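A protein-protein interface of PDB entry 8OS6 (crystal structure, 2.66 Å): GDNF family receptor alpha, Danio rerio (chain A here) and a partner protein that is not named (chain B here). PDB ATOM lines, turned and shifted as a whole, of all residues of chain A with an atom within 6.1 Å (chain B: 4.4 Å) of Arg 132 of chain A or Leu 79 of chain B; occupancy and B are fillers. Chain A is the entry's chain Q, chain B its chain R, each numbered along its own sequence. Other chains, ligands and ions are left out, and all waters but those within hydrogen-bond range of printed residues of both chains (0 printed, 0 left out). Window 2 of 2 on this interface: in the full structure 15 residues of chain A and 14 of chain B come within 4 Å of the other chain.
The guanidinium group (NH2) of Arg 75 of chain A lies within salt-bridge range of the side-chain carboxylate (OE2) of Glu 26 of chain B (2.9 Å).
The guanidinium group (NH1) of Arg 132 of chain A is in salt-bridge range of the side-chain carboxylate (OE2) of Glu 26 of chain B, at 3.8 Å.
The backbone carbonyl oxygen (O) of Gln 135 of chain A lies within hydrogen-bond range of the side-chain hydroxyl (OH) of Tyr 85 of chain B (2.9 Å).
The side-chain carboxylate (OE1) of Glu 131 of chain A is in salt-bridge range of the guanidinium group (NH1) of Arg 134 of chain A (3.1 Å).
NH1 of Arg 134 of chain A lies within hydrogen-bond range of OE1 of Gln 135 of chain A, 2.9 Å away.
OG1 of Thr 24 of chain B lies within hydrogen-bond range of N of Glu 26 of chain B, at 3.2 Å.
The side-chain hydroxyl of Thr 24 of chain B sits at hydrogen-bond distance from the backbone carbonyl oxygen of Leu 79 of chain B, at 2.7 Å.
The side-chain sulfur (SG) of Cys 58 of chain A forms a disulfide with the side-chain sulfur (SG) of Cys 119 of chain A (2.0 Å).
SG of Cys 129 of chain A is disulfide-bonded to SG of Cys 58 of chain A, at 2.1 Å.
Among the printed residues, pairs that only touch across the chains: Ala 62 of chain A with Glu 26 of chain B (3.9 Å), Glu 131 of chain A with Leu 83 of chain B (3.2 Å) and Arg 132 of chain A with Leu 79 of chain B (3.9 Å).
Of the printed residues of chain B, Arg 132 of chain A touches Glu 26 and Leu 79.
Printed residues of chain B within 4 Å of Gln 135 of chain A: Tyr 85 (2.9 Å).
Of the printed residues of chain A, Tyr 85 of chain B touches Gln 135 (2.9 Å).
The nearest residue of chain A that does not touch Leu 79 of chain B is Arg 75 of chain A (4.1 Å).
Of the 8 printed residues of chain B, 4 touch a printed residue of chain A.
Printed residues of chain B that touch a printed residue of chain A: Glu 26, Leu 79, Leu 83 and Tyr 85.
Hydrophobic or aromatic side chains of chain B within 4 Å of the printed part of chain A: Leu 79, Leu 83 and Tyr 85.
Of the 18 printed residues of chain A, 5 touch a printed residue of chain B.
Hydrophobic or aromatic side chains of chain A that line the printed part of chain B: Ala 62.
Among the printed residues, 6 pairs touch across the chains.
Among the printed residues, Asp or Glu carboxylates within 4 Å of a Lys or Arg side-chain nitrogen of the other chain: Arg 75 of chain A with Glu 26 of chain B and Arg 132 of chain A with Glu 26 of chain B.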
ATOM      1  N   ASN A  56      -4.438  -8.164   0.464  1.00  0.00           N
ATOM      2  CA  ASN A  56      -4.053  -6.962  -0.265  1.00  0.00           C
ATOM      3  C   ASN A  56      -2.534  -6.818  -0.302  1.00  0.00           C
ATOM      4  O   ASN A  56      -1.902  -6.564   0.722  1.00  0.00           O
ATOM      5  CB  ASN A  56      -4.688  -5.723   0.373  1.00  0.00           C
ATOM      6  CG  ASN A  56      -4.427  -4.455  -0.420  1.00  0.00           C
ATOM      7  OD1 ASN A  56      -3.326  -4.239  -0.928  1.00  0.00           O
ATOM      8  ND2 ASN A  56      -5.444  -3.607  -0.532  1.00  0.00           N
ATOM      9  N   CYS A  58      -0.959  -4.421  -1.954  1.00  0.00           N
ATOM     10  CA  CYS A  58      -0.632  -3.003  -1.858  1.00  0.00           C
ATOM     11  C   CYS A  58      -0.479  -2.571  -0.402  1.00  0.00           C
ATOM     12  O   CYS A  58       0.441  -1.816  -0.064  1.00  0.00           O
ATOM     13  CB  CYS A  58      -1.713  -2.174  -2.555  1.00  0.00           C
ATOM     14  SG  CYS A  58      -1.732  -2.236  -4.380  1.00  0.00           S
ATOM     15  N   LEU A  59      -1.368  -3.042   0.476  1.00  0.00           N
ATOM     16  CA  LEU A  59      -1.286  -2.666   1.885  1.00  0.00           C
ATOM     17  C   LEU A  59      -0.120  -3.360   2.577  1.00  0.00           C
ATOM     18  O   LEU A  59       0.617  -2.728   3.343  1.00  0.00           O
ATOM     19  CB  LEU A  59      -2.601  -2.999   2.588  1.00  0.00           C
ATOM     20  CG  LEU A  59      -2.619  -2.890   4.114  1.00  0.00           C
ATOM     21  CD1 LEU A  59      -2.347  -1.466   4.574  1.00  0.00           C
ATOM     22  CD2 LEU A  59      -3.956  -3.385   4.652  1.00  0.00           C
ATOM     23  N   ASN A  60       0.061  -4.659   2.326  1.00  0.00           N
ATOM     24  CA  ASN A  60       1.178  -5.381   2.927  1.00  0.00           C
ATOM     25  C   ASN A  60       2.507  -4.698   2.642  1.00  0.00           C
ATOM     26  O   ASN A  60       3.423  -4.745   3.472  1.00  0.00           O
ATOM     27  CB  ASN A  60       1.204  -6.822   2.413  1.00  0.00           C
ATOM     28  CG  ASN A  60      -0.041  -7.599   2.792  1.00  0.00           C
ATOM     29  OD1 ASN A  60      -0.932  -7.074   3.460  1.00  0.00           O
ATOM     30  ND2 ASN A  60      -0.115  -8.852   2.359  1.00  0.00           N
ATOM     31  N   ALA A  62       2.896  -1.379   2.277  1.00  0.00           N
ATOM     32  CA  ALA A  62       2.946  -0.203   3.140  1.00  0.00           C
ATOM     33  C   ALA A  62       3.372  -0.576   4.554  1.00  0.00           C
ATOM     34  O   ALA A  62       4.190   0.119   5.169  1.00  0.00           O
ATOM     35  CB  ALA A  62       1.585   0.492   3.156  1.00  0.00           C
ATOM     36  N   ARG A  75       9.316   7.929   3.842  1.00  0.00           N
ATOM     37  CA  ARG A  75       7.912   7.975   3.450  1.00  0.00           C
ATOM     38  C   ARG A  75       7.225   9.182   4.076  1.00  0.00           C
ATOM     39  O   ARG A  75       6.478   9.902   3.405  1.00  0.00           O
ATOM     40  CB  ARG A  75       7.195   6.685   3.848  1.00  0.00           C
ATOM     41  CG  ARG A  75       5.763   6.610   3.329  1.00  0.00           C
ATOM     42  CD  ARG A  75       4.981   5.451   3.932  1.00  0.00           C
ATOM     43  NE  ARG A  75       3.569   5.520   3.570  1.00  0.00           N
ATOM     44  CZ  ARG A  75       2.634   4.698   4.025  1.00  0.00           C
ATOM     45  NH1 ARG A  75       2.922   3.719   4.868  1.00  0.00           N
ATOM     46  NH2 ARG A  75       1.376   4.863   3.626  1.00  0.00           N
ATOM     47  N   MET A 116       5.996  -0.666  -3.175  1.00  0.00           N
ATOM     48  CA  MET A 116       4.778   0.112  -2.993  1.00  0.00           C
ATOM     49  C   MET A 116       4.258   0.681  -4.309  1.00  0.00           C
ATOM     50  O   MET A 116       3.049   0.645  -4.563  1.00  0.00           O
ATOM     51  CB  MET A 116       5.025   1.252  -1.999  1.00  0.00           C
ATOM     52  CG  MET A 116       5.299   0.793  -0.572  1.00  0.00           C
ATOM     53  SD  MET A 116       5.719   2.144   0.553  1.00  0.00           S
ATOM     54  CE  MET A 116       4.105   2.846   0.883  1.00  0.00           C
ATOM     55  N   CYS A 119       2.758  -2.335  -6.586  1.00  0.00           N
ATOM     56  CA  CYS A 119       2.104  -3.400  -5.835  1.00  0.00           C
ATOM     57  C   CYS A 119       1.190  -4.213  -6.745  1.00  0.00           C
ATOM     58  O   CYS A 119       0.393  -3.657  -7.505  1.00  0.00           O
ATOM     59  CB  CYS A 119       1.317  -2.830  -4.643  1.00  0.00           C
ATOM     60  SG  CYS A 119       0.096  -1.490  -4.925  1.00  0.00           S
ATOM     61  N   SER A 127     -10.421  -1.907  -7.189  1.00  0.00           N
ATOM     62  CA  SER A 127     -10.213  -2.461  -5.862  1.00  0.00           C
ATOM     63  C   SER A 127      -9.541  -1.430  -4.958  1.00  0.00           C
ATOM     64  O   SER A 127      -9.144  -0.343  -5.389  1.00  0.00           O
ATOM     65  CB  SER A 127      -9.363  -3.728  -5.937  1.00  0.00           C
ATOM     66  OG  SER A 127      -8.982  -4.158  -4.641  1.00  0.00           O
ATOM     67  N   ALA A 128      -9.411  -1.787  -3.680  1.00  0.00           N
ATOM     68  CA  ALA A 128      -8.771  -0.882  -2.733  1.00  0.00           C
ATOM     69  C   ALA A 128      -7.264  -0.814  -2.964  1.00  0.00           C
ATOM     70  O   ALA A 128      -6.675   0.271  -2.903  1.00  0.00           O
ATOM     71  CB  ALA A 128      -9.083  -1.315  -1.302  1.00  0.00           C
ATOM     72  N   CYS A 129      -6.622  -1.957  -3.232  1.00  0.00           N
ATOM     73  CA  CYS A 129      -5.195  -1.936  -3.550  1.00  0.00           C
ATOM     74  C   CYS A 129      -4.918  -1.006  -4.723  1.00  0.00           C
ATOM     75  O   CYS A 129      -3.963  -0.222  -4.691  1.00  0.00           O
ATOM     76  CB  CYS A 129      -4.689  -3.356  -3.842  1.00  0.00           C
ATOM     77  SG  CYS A 129      -3.199  -3.562  -4.936  1.00  0.00           S
ATOM     78  N   SER A 130      -5.753  -1.070  -5.765  1.00  0.00           N
ATOM     79  CA  SER A 130      -5.540  -0.214  -6.927  1.00  0.00           C
ATOM     80  C   SER A 130      -5.614   1.260  -6.554  1.00  0.00           C
ATOM     81  O   SER A 130      -4.897   2.084  -7.133  1.00  0.00           O
ATOM     82  CB  SER A 130      -6.567  -0.535  -8.013  1.00  0.00           C
ATOM     83  OG  SER A 130      -7.822   0.050  -7.714  1.00  0.00           O
ATOM     84  N   GLU A 131      -6.470   1.612  -5.592  1.00  0.00           N
ATOM     85  CA  GLU A 131      -6.586   3.005  -5.174  1.00  0.00           C
ATOM     86  C   GLU A 131      -5.419   3.426  -4.289  1.00  0.00           C
ATOM     87  O   GLU A 131      -4.934   4.557  -4.395  1.00  0.00           O
ATOM     88  CB  GLU A 131      -7.912   3.224  -4.445  1.00  0.00           C
ATOM     89  CG  GLU A 131      -9.018   3.763  -5.332  1.00  0.00           C
ATOM     90  CD  GLU A 131      -8.716   5.156  -5.851  1.00  0.00           C
ATOM     91  OE1 GLU A 131      -7.714   5.754  -5.403  1.00  0.00           O
ATOM     92  OE2 GLU A 131      -9.479   5.651  -6.706  1.00  0.00           O
ATOM     93  N   ARG A 132      -4.962   2.535  -3.408  1.00  0.00           N
ATOM     94  CA  ARG A 132      -3.776   2.827  -2.609  1.00  0.00           C
ATOM     95  C   ARG A 132      -2.576   3.108  -3.503  1.00  0.00           C
ATOM     96  O   ARG A 132      -1.841   4.079  -3.294  1.00  0.00           O
ATOM     97  CB  ARG A 132      -3.486   1.659  -1.666  1.00  0.00           C
ATOM     98  CG  ARG A 132      -2.062   1.618  -1.137  1.00  0.00           C
ATOM     99  CD  ARG A 132      -1.890   0.524  -0.094  1.00  0.00           C
ATOM    100  NE  ARG A 132      -2.654   0.806   1.116  1.00  0.00           N
ATOM    101  CZ  ARG A 132      -2.222   1.563   2.116  1.00  0.00           C
ATOM    102  NH1 ARG A 132      -1.028   2.134   2.087  1.00  0.00           N
ATOM    103  NH2 ARG A 132      -3.011   1.757   3.170  1.00  0.00           N
ATOM    104  N   ARG A 133      -2.362   2.256  -4.507  1.00  0.00           N
ATOM    105  CA  ARG A 133      -1.251   2.456  -5.430  1.00  0.00           C
ATOM    106  C   ARG A 133      -1.316   3.831  -6.078  1.00  0.00           C
ATOM    107  O   ARG A 133      -0.290   4.505  -6.232  1.00  0.00           O
ATOM    108  CB  ARG A 133      -1.275   1.358  -6.493  1.00  0.00           C
ATOM    109  CG  ARG A 133      -0.004   1.228  -7.303  1.00  0.00           C
ATOM    110  CD  ARG A 133      -0.087   0.012  -8.209  1.00  0.00           C
ATOM    111  NE  ARG A 133      -1.218   0.091  -9.125  1.00  0.00           N
ATOM    112  CZ  ARG A 133      -1.754  -0.954  -9.743  1.00  0.00           C
ATOM    113  NH1 ARG A 133      -1.309  -2.181  -9.534  1.00  0.00           N
ATOM    114  NH2 ARG A 133      -2.763  -0.762 -10.587  1.00  0.00           N
ATOM    115  N   ARG A 134      -2.518   4.269  -6.456  1.00  0.00           N
ATOM    116  CA  ARG A 134      -2.664   5.551  -7.136  1.00  0.00           C
ATOM    117  C   ARG A 134      -2.287   6.715  -6.228  1.00  0.00           C
ATOM    118  O   ARG A 134      -1.819   7.750  -6.715  1.00  0.00           O
ATOM    119  CB  ARG A 134      -4.103   5.706  -7.633  1.00  0.00           C
ATOM    120  CG  ARG A 134      -4.254   6.531  -8.900  1.00  0.00           C
ATOM    121  CD  ARG A 134      -5.722   6.763  -9.238  1.00  0.00           C
ATOM    122  NE  ARG A 134      -6.073   8.174  -9.124  1.00  0.00           N
ATOM    123  CZ  ARG A 134      -6.369   8.784  -7.985  1.00  0.00           C
ATOM    124  NH1 ARG A 134      -6.407   8.129  -6.836  1.00  0.00           N
ATOM    125  NH2 ARG A 134      -6.629  10.089  -7.998  1.00  0.00           N
ATOM    126  N   GLN A 135      -2.476   6.563  -4.916  1.00  0.00           N
ATOM    127  CA  GLN A 135      -2.185   7.610  -3.945  1.00  0.00           C
ATOM    128  C   GLN A 135      -0.741   7.589  -3.460  1.00  0.00           C
ATOM    129  O   GLN A 135      -0.388   8.367  -2.568  1.00  0.00           O
ATOM    130  CB  GLN A 135      -3.123   7.485  -2.739  1.00  0.00           C
ATOM    131  CG  GLN A 135      -4.580   7.803  -3.037  1.00  0.00           C
ATOM    132  CD  GLN A 135      -4.780   9.220  -3.542  1.00  0.00           C
ATOM    133  OE1 GLN A 135      -5.580   9.459  -4.446  1.00  0.00           O
ATOM    134  NE2 GLN A 135      -4.053  10.168  -2.958  1.00  0.00           N
ATOM    135  N   THR A 136       0.103   6.724  -4.027  1.00  0.00           N
ATOM    136  CA  THR A 136       1.465   6.587  -3.520  1.00  0.00           C
ATOM    137  C   THR A 136       2.248   7.887  -3.662  1.00  0.00           C
ATOM    138  O   THR A 136       2.966   8.290  -2.740  1.00  0.00           O
ATOM    139  CB  THR A 136       2.185   5.452  -4.249  1.00  0.00           C
ATOM    140  OG1 THR A 136       1.566   4.200  -3.925  1.00  0.00           O
ATOM    141  CG2 THR A 136       3.652   5.408  -3.851  1.00  0.00           C
ATOM    142  N   THR B  24      -7.628   2.884   9.966  1.00  0.00           N
ATOM    143  CA  THR B  24      -6.629   2.356   9.048  1.00  0.00           C
ATOM    144  C   THR B  24      -6.190   0.978   9.517  1.00  0.00           C
ATOM    145  O   THR B  24      -6.298   0.640  10.700  1.00  0.00           O
ATOM    146  CB  THR B  24      -5.416   3.290   8.944  1.00  0.00           C
ATOM    147  OG1 THR B  24      -4.490   2.776   7.980  1.00  0.00           O
ATOM    148  CG2 THR B  24      -4.719   3.417  10.296  1.00  0.00           C
ATOM    149  N   GLU B  26      -2.990   0.119   8.893  1.00  0.00           N
ATOM    150  CA  GLU B  26      -1.542   0.247   8.933  1.00  0.00           C
ATOM    151  C   GLU B  26      -1.005  -0.219  10.284  1.00  0.00           C
ATOM    152  O   GLU B  26      -1.748  -0.422  11.249  1.00  0.00           O
ATOM    153  CB  GLU B  26      -1.125   1.692   8.662  1.00  0.00           C
ATOM    154  CG  GLU B  26      -1.298   2.135   7.215  1.00  0.00           C
ATOM    155  CD  GLU B  26       0.027   2.403   6.517  1.00  0.00           C
ATOM    156  OE1 GLU B  26       1.059   1.840   6.941  1.00  0.00           O
ATOM    157  OE2 GLU B  26       0.033   3.183   5.540  1.00  0.00           O
ATOM    158  N   PHE B  78       0.654   7.582   7.519  1.00  0.00           N
ATOM    159  CA  PHE B  78      -0.151   6.434   7.130  1.00  0.00           C
ATOM    160  C   PHE B  78      -1.366   6.905   6.344  1.00  0.00           C
ATOM    161  O   PHE B  78      -1.732   8.083   6.370  1.00  0.00           O
ATOM    162  CB  PHE B  78      -0.586   5.618   8.354  1.00  0.00           C
ATOM    163  CG  PHE B  78      -1.270   6.431   9.413  1.00  0.00           C
ATOM    164  CD1 PHE B  78      -2.643   6.598   9.399  1.00  0.00           C
ATOM    165  CD2 PHE B  78      -0.539   7.024  10.425  1.00  0.00           C
ATOM    166  CE1 PHE B  78      -3.274   7.345  10.374  1.00  0.00           C
ATOM    167  CE2 PHE B  78      -1.163   7.772  11.402  1.00  0.00           C
ATOM    168  CZ  PHE B  78      -2.533   7.932  11.377  1.00  0.00           C
ATOM    169  N   LEU B  79      -1.987   5.960   5.640  1.00  0.00           N
ATOM    170  CA  LEU B  79      -3.167   6.212   4.824  1.00  0.00           C
ATOM    171  C   LEU B  79      -4.373   5.518   5.443  1.00  0.00           C
ATOM    172  O   LEU B  79      -4.288   4.348   5.833  1.00  0.00           O
ATOM    173  CB  LEU B  79      -2.957   5.715   3.394  1.00  0.00           C
ATOM    174  CG  LEU B  79      -4.050   6.075   2.388  1.00  0.00           C
ATOM    175  CD1 LEU B  79      -4.024   7.567   2.086  1.00  0.00           C
ATOM    176  CD2 LEU B  79      -3.895   5.260   1.111  1.00  0.00           C
ATOM    177  N   ASP B  80      -5.493   6.232   5.516  1.00  0.00           N
ATOM    178  CA  ASP B  80      -6.700   5.730   6.149  1.00  0.00           C
ATOM    179  C   ASP B  80      -7.637   5.123   5.106  1.00  0.00           C
ATOM    180  O   ASP B  80      -7.372   5.136   3.901  1.00  0.00           O
ATOM    181  CB  ASP B  80      -7.397   6.847   6.932  1.00  0.00           C
ATOM    182  CG  ASP B  80      -7.836   7.999   6.048  1.00  0.00           C
ATOM    183  OD1 ASP B  80      -7.545   7.965   4.835  1.00  0.00           O
ATOM    184  OD2 ASP B  80      -8.476   8.938   6.569  1.00  0.00           O
ATOM    185  N   LEU B  83      -8.835   7.164   2.092  1.00  0.00           N
ATOM    186  CA  LEU B  83      -7.800   7.616   1.162  1.00  0.00           C
ATOM    187  C   LEU B  83      -7.327   9.026   1.505  1.00  0.00           C
ATOM    188  O   LEU B  83      -7.053   9.848   0.627  1.00  0.00           O
ATOM    189  CB  LEU B  83      -8.293   7.540  -0.284  1.00  0.00           C
ATOM    190  CG  LEU B  83      -8.405   6.134  -0.881  1.00  0.00           C
ATOM    191  CD1 LEU B  83      -9.424   5.280  -0.136  1.00  0.00           C
ATOM    192  CD2 LEU B  83      -8.750   6.211  -2.367  1.00  0.00           C
ATOM    193  N   GLU B  84      -7.229   9.306   2.802  1.00  0.00           N
ATOM    194  CA  GLU B  84      -6.698  10.562   3.313  1.00  0.00           C
ATOM    195  C   GLU B  84      -5.436  10.270   4.113  1.00  0.00           C
ATOM    196  O   GLU B  84      -5.386   9.303   4.881  1.00  0.00           O
ATOM    197  CB  GLU B  84      -7.729  11.285   4.188  1.00  0.00           C
ATOM    198  CG  GLU B  84      -7.320  12.689   4.608  1.00  0.00           C
ATOM    199  CD  GLU B  84      -8.282  13.307   5.610  1.00  0.00           C
ATOM    200  OE1 GLU B  84      -9.344  12.703   5.872  1.00  0.00           O
ATOM    201  OE2 GLU B  84      -7.970  14.397   6.139  1.00  0.00           O
ATOM    202  N   TYR B  85      -4.418  11.102   3.931  1.00  0.00           N
ATOM    203  CA  TYR B  85      -3.137  10.898   4.590  1.00  0.00           C
ATOM    204  C   TYR B  85      -3.101  11.595   5.945  1.00  0.00           C
ATOM    205  O   TYR B  85      -3.694  12.661   6.138  1.00  0.00           O
ATOM    206  CB  TYR B  85      -1.996  11.410   3.711  1.00  0.00           C
ATOM    207  CG  TYR B  85      -1.433  10.373   2.765  1.00  0.00           C
ATOM    208  CD1 TYR B  85      -1.034   9.125   3.227  1.00  0.00           C
ATOM    209  CD2 TYR B  85      -1.301  10.640   1.409  1.00  0.00           C
ATOM    210  CE1 TYR B  85      -0.518   8.177   2.369  1.00  0.00           C
ATOM    211  CE2 TYR B  85      -0.786   9.696   0.542  1.00  0.00           C
ATOM    212  CZ  TYR B  85      -0.396   8.465   1.028  1.00  0.00           C
ATOM    213  OH  TYR B  85       0.119   7.516   0.174  1.00  0.00           O
